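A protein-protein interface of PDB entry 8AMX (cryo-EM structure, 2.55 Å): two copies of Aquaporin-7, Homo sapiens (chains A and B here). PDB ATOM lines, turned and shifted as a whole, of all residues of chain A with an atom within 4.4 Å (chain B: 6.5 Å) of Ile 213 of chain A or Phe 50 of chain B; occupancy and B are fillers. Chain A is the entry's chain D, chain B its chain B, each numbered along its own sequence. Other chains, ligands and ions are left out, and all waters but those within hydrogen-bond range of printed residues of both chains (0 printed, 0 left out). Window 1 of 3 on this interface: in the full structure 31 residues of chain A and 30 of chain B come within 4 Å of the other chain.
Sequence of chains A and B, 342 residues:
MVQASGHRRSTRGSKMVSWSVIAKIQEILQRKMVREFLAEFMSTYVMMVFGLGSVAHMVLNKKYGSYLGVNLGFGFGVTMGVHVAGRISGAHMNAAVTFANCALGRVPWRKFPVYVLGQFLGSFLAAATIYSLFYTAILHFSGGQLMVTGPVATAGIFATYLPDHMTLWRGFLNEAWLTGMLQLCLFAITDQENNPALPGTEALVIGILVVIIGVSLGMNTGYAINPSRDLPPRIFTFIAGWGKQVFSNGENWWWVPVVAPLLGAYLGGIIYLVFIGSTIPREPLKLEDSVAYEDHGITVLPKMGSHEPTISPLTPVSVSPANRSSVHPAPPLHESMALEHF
No position is printed for both chains. Of the 12 pairs that touch across the chains among the printed residues, none has its exchanged pair printed and touching as well.
OG of Ser 216 of chain A sits at hydrogen-bond distance from O of Phe 50 of chain B (2.9 Å). OG of Ser 54 of chain B lies within hydrogen-bond range of OG of Ser 216 of chain A (3.0 Å). A ring nitrogen (ND1) of His 57 of chain B is in hydrogen-bond range of the backbone carbonyl oxygen of Ser 216 of chain A. O of Ser 216 of chain A lies close to O of Gly 53 of chain B, 3.2 Å away.
Among the printed residues, pairs that only touch across the chains: Leu 209 of chain A with Met 80 of chain B (3.7 Å), Ile 212 of chain A with Phe 76 of chain B (3.5 Å), Ile 213 of chain A with Phe 50 of chain B (3.95 Å), Val 215 of chain A with Ser 54 of chain B (3.9 Å), Val 215 of chain A with His 57 of chain B (3.6 Å), Val 215 of chain A with Gly 69 of chain B (3.5 Å), Leu 217 of chain A with His 57 of chain B (3.7 Å) and Gly 218 of chain A with His 57 of chain B (3.5 Å).
Ile 213 of chain A touches just one residue of chain B: Phe 50 (3.95 Å). Of chain A, only Ile 213 (3.95 Å) and Ser 216 (2.9 Å) come within 4 Å of Phe 50 of chain B. Of the printed residues of chain A, His 57 of chain B touches Val 215, Ser 216, Leu 217 and Gly 218. Printed residues of chain A within 4 Å of Gly 69 of chain B: Val 215 (3.5 Å). Printed residues of chain A within 4 Å of Phe 76 of chain B: Ile 212. Printed residues of chain B within 4 Å of Leu 209 of chain A: Met 80 (3.7 Å). The nearest residue of chain B that does not touch Ile 213 of chain A is His 57 of chain B (6.4 Å).
Of the 13 printed residues of chain A, 7 touch a printed residue of chain B. Hydrophobic or aromatic side chains of chain A within 4 Å of the printed part of chain B: Leu 209, Ile 212, Ile 213 and Val 215. Of the 21 printed residues of chain B, 7 touch a printed residue of chain A. Among the printed residues, 12 pairs touch across the chains.
O of Phe 50 of chain B lies within hydrogen-bond range of OG of Ser 54 of chain B, at 3.4 Å. A ring nitrogen (ND1) of His 57 of chain B is in hydrogen-bond range of the backbone carbonyl oxygen (O) of Gly 53 of chain B. The side-chain hydroxyl (OG) of Ser 54 of chain B lies within hydrogen-bond range of the backbone carbonyl oxygen (O) of Gly 69 of chain B (3.3 Å). The backbone carbonyl oxygen (O) of Ile 212 of chain A lies within hydrogen-bond range of the side-chain hydroxyl (OG) of Ser 216 of chain A (3.4 Å).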
ATOM      1  N   MET A 181      10.964  14.759 -24.889  1.00  0.00           N
ATOM      2  CA  MET A 181      11.352  16.167 -24.931  1.00  0.00           C
ATOM      3  C   MET A 181      11.681  16.605 -26.352  1.00  0.00           C
ATOM      4  O   MET A 181      11.258  17.686 -26.796  1.00  0.00           O
ATOM      5  CB  MET A 181      12.555  16.412 -24.020  1.00  0.00           C
ATOM      6  CG  MET A 181      12.297  16.200 -22.542  1.00  0.00           C
ATOM      7  SD  MET A 181      11.416  17.564 -21.764  1.00  0.00           S
ATOM      8  CE  MET A 181      12.600  18.886 -21.969  1.00  0.00           C
ATOM      9  N   LEU A 182      12.435  15.778 -27.081  1.00  0.00           N
ATOM     10  CA  LEU A 182      12.791  16.115 -28.455  1.00  0.00           C
ATOM     11  C   LEU A 182      11.551  16.309 -29.317  1.00  0.00           C
ATOM     12  O   LEU A 182      11.454  17.283 -30.071  1.00  0.00           O
ATOM     13  CB  LEU A 182      13.689  15.029 -29.044  1.00  0.00           C
ATOM     14  CG  LEU A 182      13.893  15.034 -30.559  1.00  0.00           C
ATOM     15  CD1 LEU A 182      14.890  16.091 -30.976  1.00  0.00           C
ATOM     16  CD2 LEU A 182      14.316  13.665 -31.048  1.00  0.00           C
ATOM     17  N   LEU A 209      18.547  22.725 -30.661  1.00  0.00           N
ATOM     18  CA  LEU A 209      17.791  21.832 -29.787  1.00  0.00           C
ATOM     19  C   LEU A 209      18.536  20.521 -29.562  1.00  0.00           C
ATOM     20  O   LEU A 209      18.659  20.046 -28.426  1.00  0.00           O
ATOM     21  CB  LEU A 209      16.409  21.568 -30.386  1.00  0.00           C
ATOM     22  CG  LEU A 209      15.627  20.375 -29.829  1.00  0.00           C
ATOM     23  CD1 LEU A 209      15.201  20.615 -28.394  1.00  0.00           C
ATOM     24  CD2 LEU A 209      14.437  20.048 -30.703  1.00  0.00           C
ATOM     25  N   VAL A 210      19.048  19.926 -30.640  1.00  0.00           N
ATOM     26  CA  VAL A 210      19.790  18.671 -30.506  1.00  0.00           C
ATOM     27  C   VAL A 210      21.082  18.887 -29.715  1.00  0.00           C
ATOM     28  O   VAL A 210      21.477  18.047 -28.890  1.00  0.00           O
ATOM     29  CB  VAL A 210      20.051  18.061 -31.894  1.00  0.00           C
ATOM     30  CG1 VAL A 210      20.773  16.734 -31.776  1.00  0.00           C
ATOM     31  CG2 VAL A 210      18.741  17.883 -32.628  1.00  0.00           C
ATOM     32  N   VAL A 211      21.745  20.026 -29.936  1.00  0.00           N
ATOM     33  CA  VAL A 211      22.972  20.341 -29.206  1.00  0.00           C
ATOM     34  C   VAL A 211      22.711  20.376 -27.704  1.00  0.00           C
ATOM     35  O   VAL A 211      23.466  19.803 -26.913  1.00  0.00           O
ATOM     36  CB  VAL A 211      23.570  21.671 -29.703  1.00  0.00           C
ATOM     37  CG1 VAL A 211      24.657  22.153 -28.764  1.00  0.00           C
ATOM     38  CG2 VAL A 211      24.132  21.523 -31.098  1.00  0.00           C
ATOM     39  N   ILE A 212      21.636  21.047 -27.286  1.00  0.00           N
ATOM     40  CA  ILE A 212      21.420  21.187 -25.846  1.00  0.00           C
ATOM     41  C   ILE A 212      20.821  19.925 -25.239  1.00  0.00           C
ATOM     42  O   ILE A 212      20.988  19.683 -24.040  1.00  0.00           O
ATOM     43  CB  ILE A 212      20.565  22.421 -25.510  1.00  0.00           C
ATOM     44  CG1 ILE A 212      19.150  22.288 -26.069  1.00  0.00           C
ATOM     45  CG2 ILE A 212      21.253  23.676 -25.996  1.00  0.00           C
ATOM     46  CD1 ILE A 212      18.221  23.365 -25.612  1.00  0.00           C
ATOM     47  N   ILE A 213      20.127  19.095 -26.022  1.00  0.00           N
ATOM     48  CA  ILE A 213      19.780  17.769 -25.514  1.00  0.00           C
ATOM     49  C   ILE A 213      21.045  16.988 -25.195  1.00  0.00           C
ATOM     50  O   ILE A 213      21.136  16.317 -24.161  1.00  0.00           O
ATOM     51  CB  ILE A 213      18.884  17.008 -26.508  1.00  0.00           C
ATOM     52  CG1 ILE A 213      17.483  17.611 -26.551  1.00  0.00           C
ATOM     53  CG2 ILE A 213      18.783  15.547 -26.115  1.00  0.00           C
ATOM     54  CD1 ILE A 213      16.571  16.925 -27.519  1.00  0.00           C
ATOM     55  N   GLY A 214      22.044  17.062 -26.075  1.00  0.00           N
ATOM     56  CA  GLY A 214      23.319  16.435 -25.764  1.00  0.00           C
ATOM     57  C   GLY A 214      24.001  17.036 -24.547  1.00  0.00           C
ATOM     58  O   GLY A 214      24.528  16.313 -23.700  1.00  0.00           O
ATOM     59  N   VAL A 215      23.992  18.365 -24.442  1.00  0.00           N
ATOM     60  CA  VAL A 215      24.699  19.050 -23.360  1.00  0.00           C
ATOM     61  C   VAL A 215      24.081  18.730 -22.002  1.00  0.00           C
ATOM     62  O   VAL A 215      24.797  18.473 -21.028  1.00  0.00           O
ATOM     63  CB  VAL A 215      24.729  20.570 -23.617  1.00  0.00           C
ATOM     64  CG1 VAL A 215      25.131  21.320 -22.363  1.00  0.00           C
ATOM     65  CG2 VAL A 215      25.683  20.902 -24.742  1.00  0.00           C
ATOM     66  N   SER A 216      22.755  18.740 -21.908  1.00  0.00           N
ATOM     67  CA  SER A 216      22.093  18.666 -20.613  1.00  0.00           C
ATOM     68  C   SER A 216      21.801  17.251 -20.136  1.00  0.00           C
ATOM     69  O   SER A 216      21.823  17.006 -18.927  1.00  0.00           O
ATOM     70  CB  SER A 216      20.779  19.448 -20.649  1.00  0.00           C
ATOM     71  OG  SER A 216      21.012  20.824 -20.852  1.00  0.00           O
ATOM     72  N   LEU A 217      21.513  16.309 -21.033  1.00  0.00           N
ATOM     73  CA  LEU A 217      20.930  15.050 -20.585  1.00  0.00           C
ATOM     74  C   LEU A 217      21.567  13.839 -21.248  1.00  0.00           C
ATOM     75  O   LEU A 217      20.942  12.779 -21.324  1.00  0.00           O
ATOM     76  CB  LEU A 217      19.422  15.026 -20.856  1.00  0.00           C
ATOM     77  CG  LEU A 217      18.581  16.248 -20.491  1.00  0.00           C
ATOM     78  CD1 LEU A 217      17.315  16.292 -21.325  1.00  0.00           C
ATOM     79  CD2 LEU A 217      18.252  16.237 -19.014  1.00  0.00           C
ATOM     80  N   GLY A 218      22.808  13.952 -21.712  1.00  0.00           N
ATOM     81  CA  GLY A 218      23.384  12.931 -22.559  1.00  0.00           C
ATOM     82  C   GLY A 218      24.426  12.002 -21.978  1.00  0.00           C
ATOM     83  O   GLY A 218      25.031  11.236 -22.738  1.00  0.00           O
ATOM     84  N   ILE A 225      18.461   8.385 -28.603  1.00  0.00           N
ATOM     85  CA  ILE A 225      17.153   8.963 -28.925  1.00  0.00           C
ATOM     86  C   ILE A 225      16.747   8.734 -30.377  1.00  0.00           C
ATOM     87  O   ILE A 225      15.897   9.450 -30.913  1.00  0.00           O
ATOM     88  CB  ILE A 225      17.099  10.468 -28.577  1.00  0.00           C
ATOM     89  CG1 ILE A 225      17.953  11.310 -29.528  1.00  0.00           C
ATOM     90  CG2 ILE A 225      17.527  10.697 -27.142  1.00  0.00           C
ATOM     91  CD1 ILE A 225      17.936  12.788 -29.234  1.00  0.00           C
ATOM     92  N   TYR B  45       8.728  24.323 -17.303  1.00  0.00           N
ATOM     93  CA  TYR B  45       9.210  22.954 -17.153  1.00  0.00           C
ATOM     94  C   TYR B  45      10.356  22.663 -18.113  1.00  0.00           C
ATOM     95  O   TYR B  45      11.394  22.121 -17.714  1.00  0.00           O
ATOM     96  CB  TYR B  45       8.059  21.970 -17.372  1.00  0.00           C
ATOM     97  CG  TYR B  45       8.479  20.522 -17.324  1.00  0.00           C
ATOM     98  CD1 TYR B  45       8.600  19.857 -16.118  1.00  0.00           C
ATOM     99  CD2 TYR B  45       8.763  19.822 -18.485  1.00  0.00           C
ATOM    100  CE1 TYR B  45       8.989  18.545 -16.070  1.00  0.00           C
ATOM    101  CE2 TYR B  45       9.156  18.507 -18.443  1.00  0.00           C
ATOM    102  CZ  TYR B  45       9.267  17.874 -17.233  1.00  0.00           C
ATOM    103  OH  TYR B  45       9.653  16.560 -17.177  1.00  0.00           O
ATOM    104  N   VAL B  46      10.188  23.028 -19.386  1.00  0.00           N
ATOM    105  CA  VAL B  46      11.224  22.759 -20.386  1.00  0.00           C
ATOM    106  C   VAL B  46      12.522  23.480 -20.023  1.00  0.00           C
ATOM    107  O   VAL B  46      13.612  22.878 -19.998  1.00  0.00           O
ATOM    108  CB  VAL B  46      10.720  23.163 -21.783  1.00  0.00           C
ATOM    109  CG1 VAL B  46      11.855  23.193 -22.784  1.00  0.00           C
ATOM    110  CG2 VAL B  46       9.626  22.221 -22.239  1.00  0.00           C
ATOM    111  N   MET B  47      12.417  24.778 -19.712  1.00  0.00           N
ATOM    112  CA  MET B  47      13.604  25.565 -19.394  1.00  0.00           C
ATOM    113  C   MET B  47      14.339  25.005 -18.181  1.00  0.00           C
ATOM    114  O   MET B  47      15.572  24.873 -18.193  1.00  0.00           O
ATOM    115  CB  MET B  47      13.195  27.022 -19.163  1.00  0.00           C
ATOM    116  CG  MET B  47      14.329  27.976 -18.849  1.00  0.00           C
ATOM    117  SD  MET B  47      14.543  28.300 -17.092  1.00  0.00           S
ATOM    118  CE  MET B  47      12.906  28.859 -16.656  1.00  0.00           C
ATOM    119  N   MET B  48      13.595  24.651 -17.130  1.00  0.00           N
ATOM    120  CA  MET B  48      14.221  24.178 -15.904  1.00  0.00           C
ATOM    121  C   MET B  48      14.845  22.802 -16.082  1.00  0.00           C
ATOM    122  O   MET B  48      15.890  22.514 -15.492  1.00  0.00           O
ATOM    123  CB  MET B  48      13.203  24.169 -14.767  1.00  0.00           C
ATOM    124  CG  MET B  48      12.846  25.545 -14.254  1.00  0.00           C
ATOM    125  SD  MET B  48      14.245  26.372 -13.498  1.00  0.00           S
ATOM    126  CE  MET B  48      14.635  25.216 -12.198  1.00  0.00           C
ATOM    127  N   VAL B  49      14.222  21.931 -16.878  1.00  0.00           N
ATOM    128  CA  VAL B  49      14.808  20.614 -17.112  1.00  0.00           C
ATOM    129  C   VAL B  49      16.161  20.756 -17.794  1.00  0.00           C
ATOM    130  O   VAL B  49      17.158  20.161 -17.362  1.00  0.00           O
ATOM    131  CB  VAL B  49      13.849  19.726 -17.925  1.00  0.00           C
ATOM    132  CG1 VAL B  49      14.583  18.529 -18.473  1.00  0.00           C
ATOM    133  CG2 VAL B  49      12.709  19.261 -17.059  1.00  0.00           C
ATOM    134  N   PHE B  50      16.230  21.584 -18.840  1.00  0.00           N
ATOM    135  CA  PHE B  50      17.515  21.772 -19.519  1.00  0.00           C
ATOM    136  C   PHE B  50      18.568  22.376 -18.582  1.00  0.00           C
ATOM    137  O   PHE B  50      19.713  21.897 -18.520  1.00  0.00           O
ATOM    138  CB  PHE B  50      17.324  22.629 -20.768  1.00  0.00           C
ATOM    139  CG  PHE B  50      16.783  21.869 -21.944  1.00  0.00           C
ATOM    140  CD1 PHE B  50      17.405  20.716 -22.386  1.00  0.00           C
ATOM    141  CD2 PHE B  50      15.644  22.299 -22.602  1.00  0.00           C
ATOM    142  CE1 PHE B  50      16.908  20.012 -23.463  1.00  0.00           C
ATOM    143  CE2 PHE B  50      15.144  21.598 -23.680  1.00  0.00           C
ATOM    144  CZ  PHE B  50      15.776  20.454 -24.109  1.00  0.00           C
ATOM    145  N   GLY B  51      18.191  23.405 -17.816  1.00  0.00           N
ATOM    146  CA  GLY B  51      19.166  24.052 -16.948  1.00  0.00           C
ATOM    147  C   GLY B  51      19.693  23.154 -15.841  1.00  0.00           C
ATOM    148  O   GLY B  51      20.908  23.065 -15.614  1.00  0.00           O
ATOM    149  N   LEU B  52      18.789  22.469 -15.135  1.00  0.00           N
ATOM    150  CA  LEU B  52      19.226  21.608 -14.042  1.00  0.00           C
ATOM    151  C   LEU B  52      19.985  20.391 -14.552  1.00  0.00           C
ATOM    152  O   LEU B  52      20.882  19.897 -13.861  1.00  0.00           O
ATOM    153  CB  LEU B  52      18.035  21.180 -13.184  1.00  0.00           C
ATOM    154  CG  LEU B  52      17.294  22.264 -12.393  1.00  0.00           C
ATOM    155  CD1 LEU B  52      16.258  21.649 -11.475  1.00  0.00           C
ATOM    156  CD2 LEU B  52      18.246  23.145 -11.609  1.00  0.00           C
ATOM    157  N   GLY B  53      19.662  19.900 -15.754  1.00  0.00           N
ATOM    158  CA  GLY B  53      20.483  18.859 -16.345  1.00  0.00           C
ATOM    159  C   GLY B  53      21.910  19.313 -16.583  1.00  0.00           C
ATOM    160  O   GLY B  53      22.859  18.569 -16.322  1.00  0.00           O
ATOM    161  N   SER B  54      22.082  20.543 -17.080  1.00  0.00           N
ATOM    162  CA  SER B  54      23.433  21.071 -17.258  1.00  0.00           C
ATOM    163  C   SER B  54      24.185  21.151 -15.932  1.00  0.00           C
ATOM    164  O   SER B  54      25.366  20.780 -15.846  1.00  0.00           O
ATOM    165  CB  SER B  54      23.374  22.447 -17.911  1.00  0.00           C
ATOM    166  OG  SER B  54      22.990  22.343 -19.263  1.00  0.00           O
ATOM    167  N   VAL B  55      23.515  21.638 -14.885  1.00  0.00           N
ATOM    168  CA  VAL B  55      24.178  21.768 -13.586  1.00  0.00           C
ATOM    169  C   VAL B  55      24.579  20.399 -13.038  1.00  0.00           C
ATOM    170  O   VAL B  55      25.677  20.231 -12.490  1.00  0.00           O
ATOM    171  CB  VAL B  55      23.286  22.537 -12.596  1.00  0.00           C
ATOM    172  CG1 VAL B  55      23.990  22.680 -11.262  1.00  0.00           C
ATOM    173  CG2 VAL B  55      22.938  23.899 -13.149  1.00  0.00           C
ATOM    174  N   HIS B  57      25.225  17.670 -14.792  1.00  0.00           N
ATOM    175  CA  HIS B  57      26.372  17.232 -15.583  1.00  0.00           C
ATOM    176  C   HIS B  57      27.664  17.837 -15.056  1.00  0.00           C
ATOM    177  O   HIS B  57      28.681  17.146 -14.946  1.00  0.00           O
ATOM    178  CB  HIS B  57      26.191  17.623 -17.050  1.00  0.00           C
ATOM    179  CG  HIS B  57      25.642  16.534 -17.914  1.00  0.00           C
ATOM    180  ND1 HIS B  57      24.357  16.057 -17.786  1.00  0.00           N
ATOM    181  CD2 HIS B  57      26.197  15.847 -18.938  1.00  0.00           C
ATOM    182  CE1 HIS B  57      24.150  15.112 -18.683  1.00  0.00           C
ATOM    183  NE2 HIS B  57      25.249  14.969 -19.399  1.00  0.00           N
ATOM    184  N   GLY B  69      28.979  24.649 -20.489  1.00  0.00           N
ATOM    185  CA  GLY B  69      27.813  23.809 -20.693  1.00  0.00           C
ATOM    186  C   GLY B  69      26.618  24.253 -19.874  1.00  0.00           C
ATOM    187  O   GLY B  69      25.483  24.196 -20.341  1.00  0.00           O
ATOM    188  N   VAL B  70      26.855  24.705 -18.642  1.00  0.00           N
ATOM    189  CA  VAL B  70      25.768  25.204 -17.803  1.00  0.00           C
ATOM    190  C   VAL B  70      25.150  26.454 -18.418  1.00  0.00           C
ATOM    191  O   VAL B  70      23.917  26.596 -18.500  1.00  0.00           O
ATOM    192  CB  VAL B  70      26.275  25.471 -16.374  1.00  0.00           C
ATOM    193  CG1 VAL B  70      25.151  25.980 -15.493  1.00  0.00           C
ATOM    194  CG2 VAL B  70      26.887  24.220 -15.786  1.00  0.00           C
ATOM    195  N   GLY B  73      23.146  25.437 -21.504  1.00  0.00           N
ATOM    196  CA  GLY B  73      21.920  24.740 -21.160  1.00  0.00           C
ATOM    197  C   GLY B  73      20.823  25.682 -20.714  1.00  0.00           C
ATOM    198  O   GLY B  73      19.705  25.638 -21.234  1.00  0.00           O
ATOM    199  N   PHE B  74      21.142  26.589 -19.788  1.00  0.00           N
ATOM    200  CA  PHE B  74      20.113  27.515 -19.315  1.00  0.00           C
ATOM    201  C   PHE B  74      19.644  28.456 -20.427  1.00  0.00           C
ATOM    202  O   PHE B  74      18.433  28.647 -20.623  1.00  0.00           O
ATOM    203  CB  PHE B  74      20.612  28.295 -18.098  1.00  0.00           C
ATOM    204  CG  PHE B  74      20.171  27.707 -16.784  1.00  0.00           C
ATOM    205  CD1 PHE B  74      18.842  27.763 -16.398  1.00  0.00           C
ATOM    206  CD2 PHE B  74      21.076  27.086 -15.943  1.00  0.00           C
ATOM    207  CE1 PHE B  74      18.426  27.214 -15.203  1.00  0.00           C
ATOM    208  CE2 PHE B  74      20.662  26.538 -14.744  1.00  0.00           C
ATOM    209  CZ  PHE B  74      19.338  26.603 -14.375  1.00  0.00           C
ATOM    210  N   PHE B  76      19.713  28.237 -23.832  1.00  0.00           N
ATOM    211  CA  PHE B  76      18.930  27.701 -24.932  1.00  0.00           C
ATOM    212  C   PHE B  76      17.717  26.901 -24.462  1.00  0.00           C
ATOM    213  O   PHE B  76      16.776  26.714 -25.247  1.00  0.00           O
ATOM    214  CB  PHE B  76      19.847  26.911 -25.858  1.00  0.00           C
ATOM    215  CG  PHE B  76      20.823  27.786 -26.601  1.00  0.00           C
ATOM    216  CD1 PHE B  76      20.389  28.950 -27.218  1.00  0.00           C
ATOM    217  CD2 PHE B  76      22.168  27.476 -26.652  1.00  0.00           C
ATOM    218  CE1 PHE B  76      21.270  29.771 -27.888  1.00  0.00           C
ATOM    219  CE2 PHE B  76      23.055  28.297 -27.325  1.00  0.00           C
ATOM    220  CZ  PHE B  76      22.602  29.446 -27.941  1.00  0.00           C
ATOM    221  N   GLY B  77      17.659  26.511 -23.185  1.00  0.00           N
ATOM    222  CA  GLY B  77      16.382  26.119 -22.619  1.00  0.00           C
ATOM    223  C   GLY B  77      15.401  27.273 -22.582  1.00  0.00           C
ATOM    224  O   GLY B  77      14.204  27.091 -22.825  1.00  0.00           O
ATOM    225  N   VAL B  78      15.894  28.479 -22.283  1.00  0.00           N
ATOM    226  CA  VAL B  78      15.045  29.666 -22.385  1.00  0.00           C
ATOM    227  C   VAL B  78      14.548  29.851 -23.816  1.00  0.00           C
ATOM    228  O   VAL B  78      13.379  30.187 -24.044  1.00  0.00           O
ATOM    229  CB  VAL B  78      15.793  30.912 -21.875  1.00  0.00           C
ATOM    230  CG1 VAL B  78      15.055  32.177 -22.268  1.00  0.00           C
ATOM    231  CG2 VAL B  78      15.950  30.854 -20.372  1.00  0.00           C
ATOM    232  N   MET B  80      14.012  27.499 -26.109  1.00  0.00           N
ATOM    233  CA  MET B  80      12.972  26.510 -26.394  1.00  0.00           C
ATOM    234  C   MET B  80      11.662  26.845 -25.684  1.00  0.00           C
ATOM    235  O   MET B  80      10.575  26.666 -26.254  1.00  0.00           O
ATOM    236  CB  MET B  80      13.457  25.114 -26.015  1.00  0.00           C
ATOM    237  CG  MET B  80      14.623  24.635 -26.855  1.00  0.00           C
ATOM    238  SD  MET B  80      14.262  24.698 -28.614  1.00  0.00           S
ATOM    239  CE  MET B  80      15.871  25.089 -29.279  1.00  0.00           C
ATOM    240  N   ILE B 130      14.575  15.715 -12.721  1.00  0.00           N
ATOM    241  CA  ILE B 130      16.032  15.635 -12.690  1.00  0.00           C
ATOM    242  C   ILE B 130      16.490  14.703 -11.576  1.00  0.00           C
ATOM    243  O   ILE B 130      17.477  13.973 -11.721  1.00  0.00           O
ATOM    244  CB  ILE B 130      16.646  17.041 -12.560  1.00  0.00           C
ATOM    245  CG1 ILE B 130      16.369  17.853 -13.824  1.00  0.00           C
ATOM    246  CG2 ILE B 130      18.141  16.967 -12.306  1.00  0.00           C
ATOM    247  CD1 ILE B 130      16.870  17.204 -15.082  1.00  0.00           C
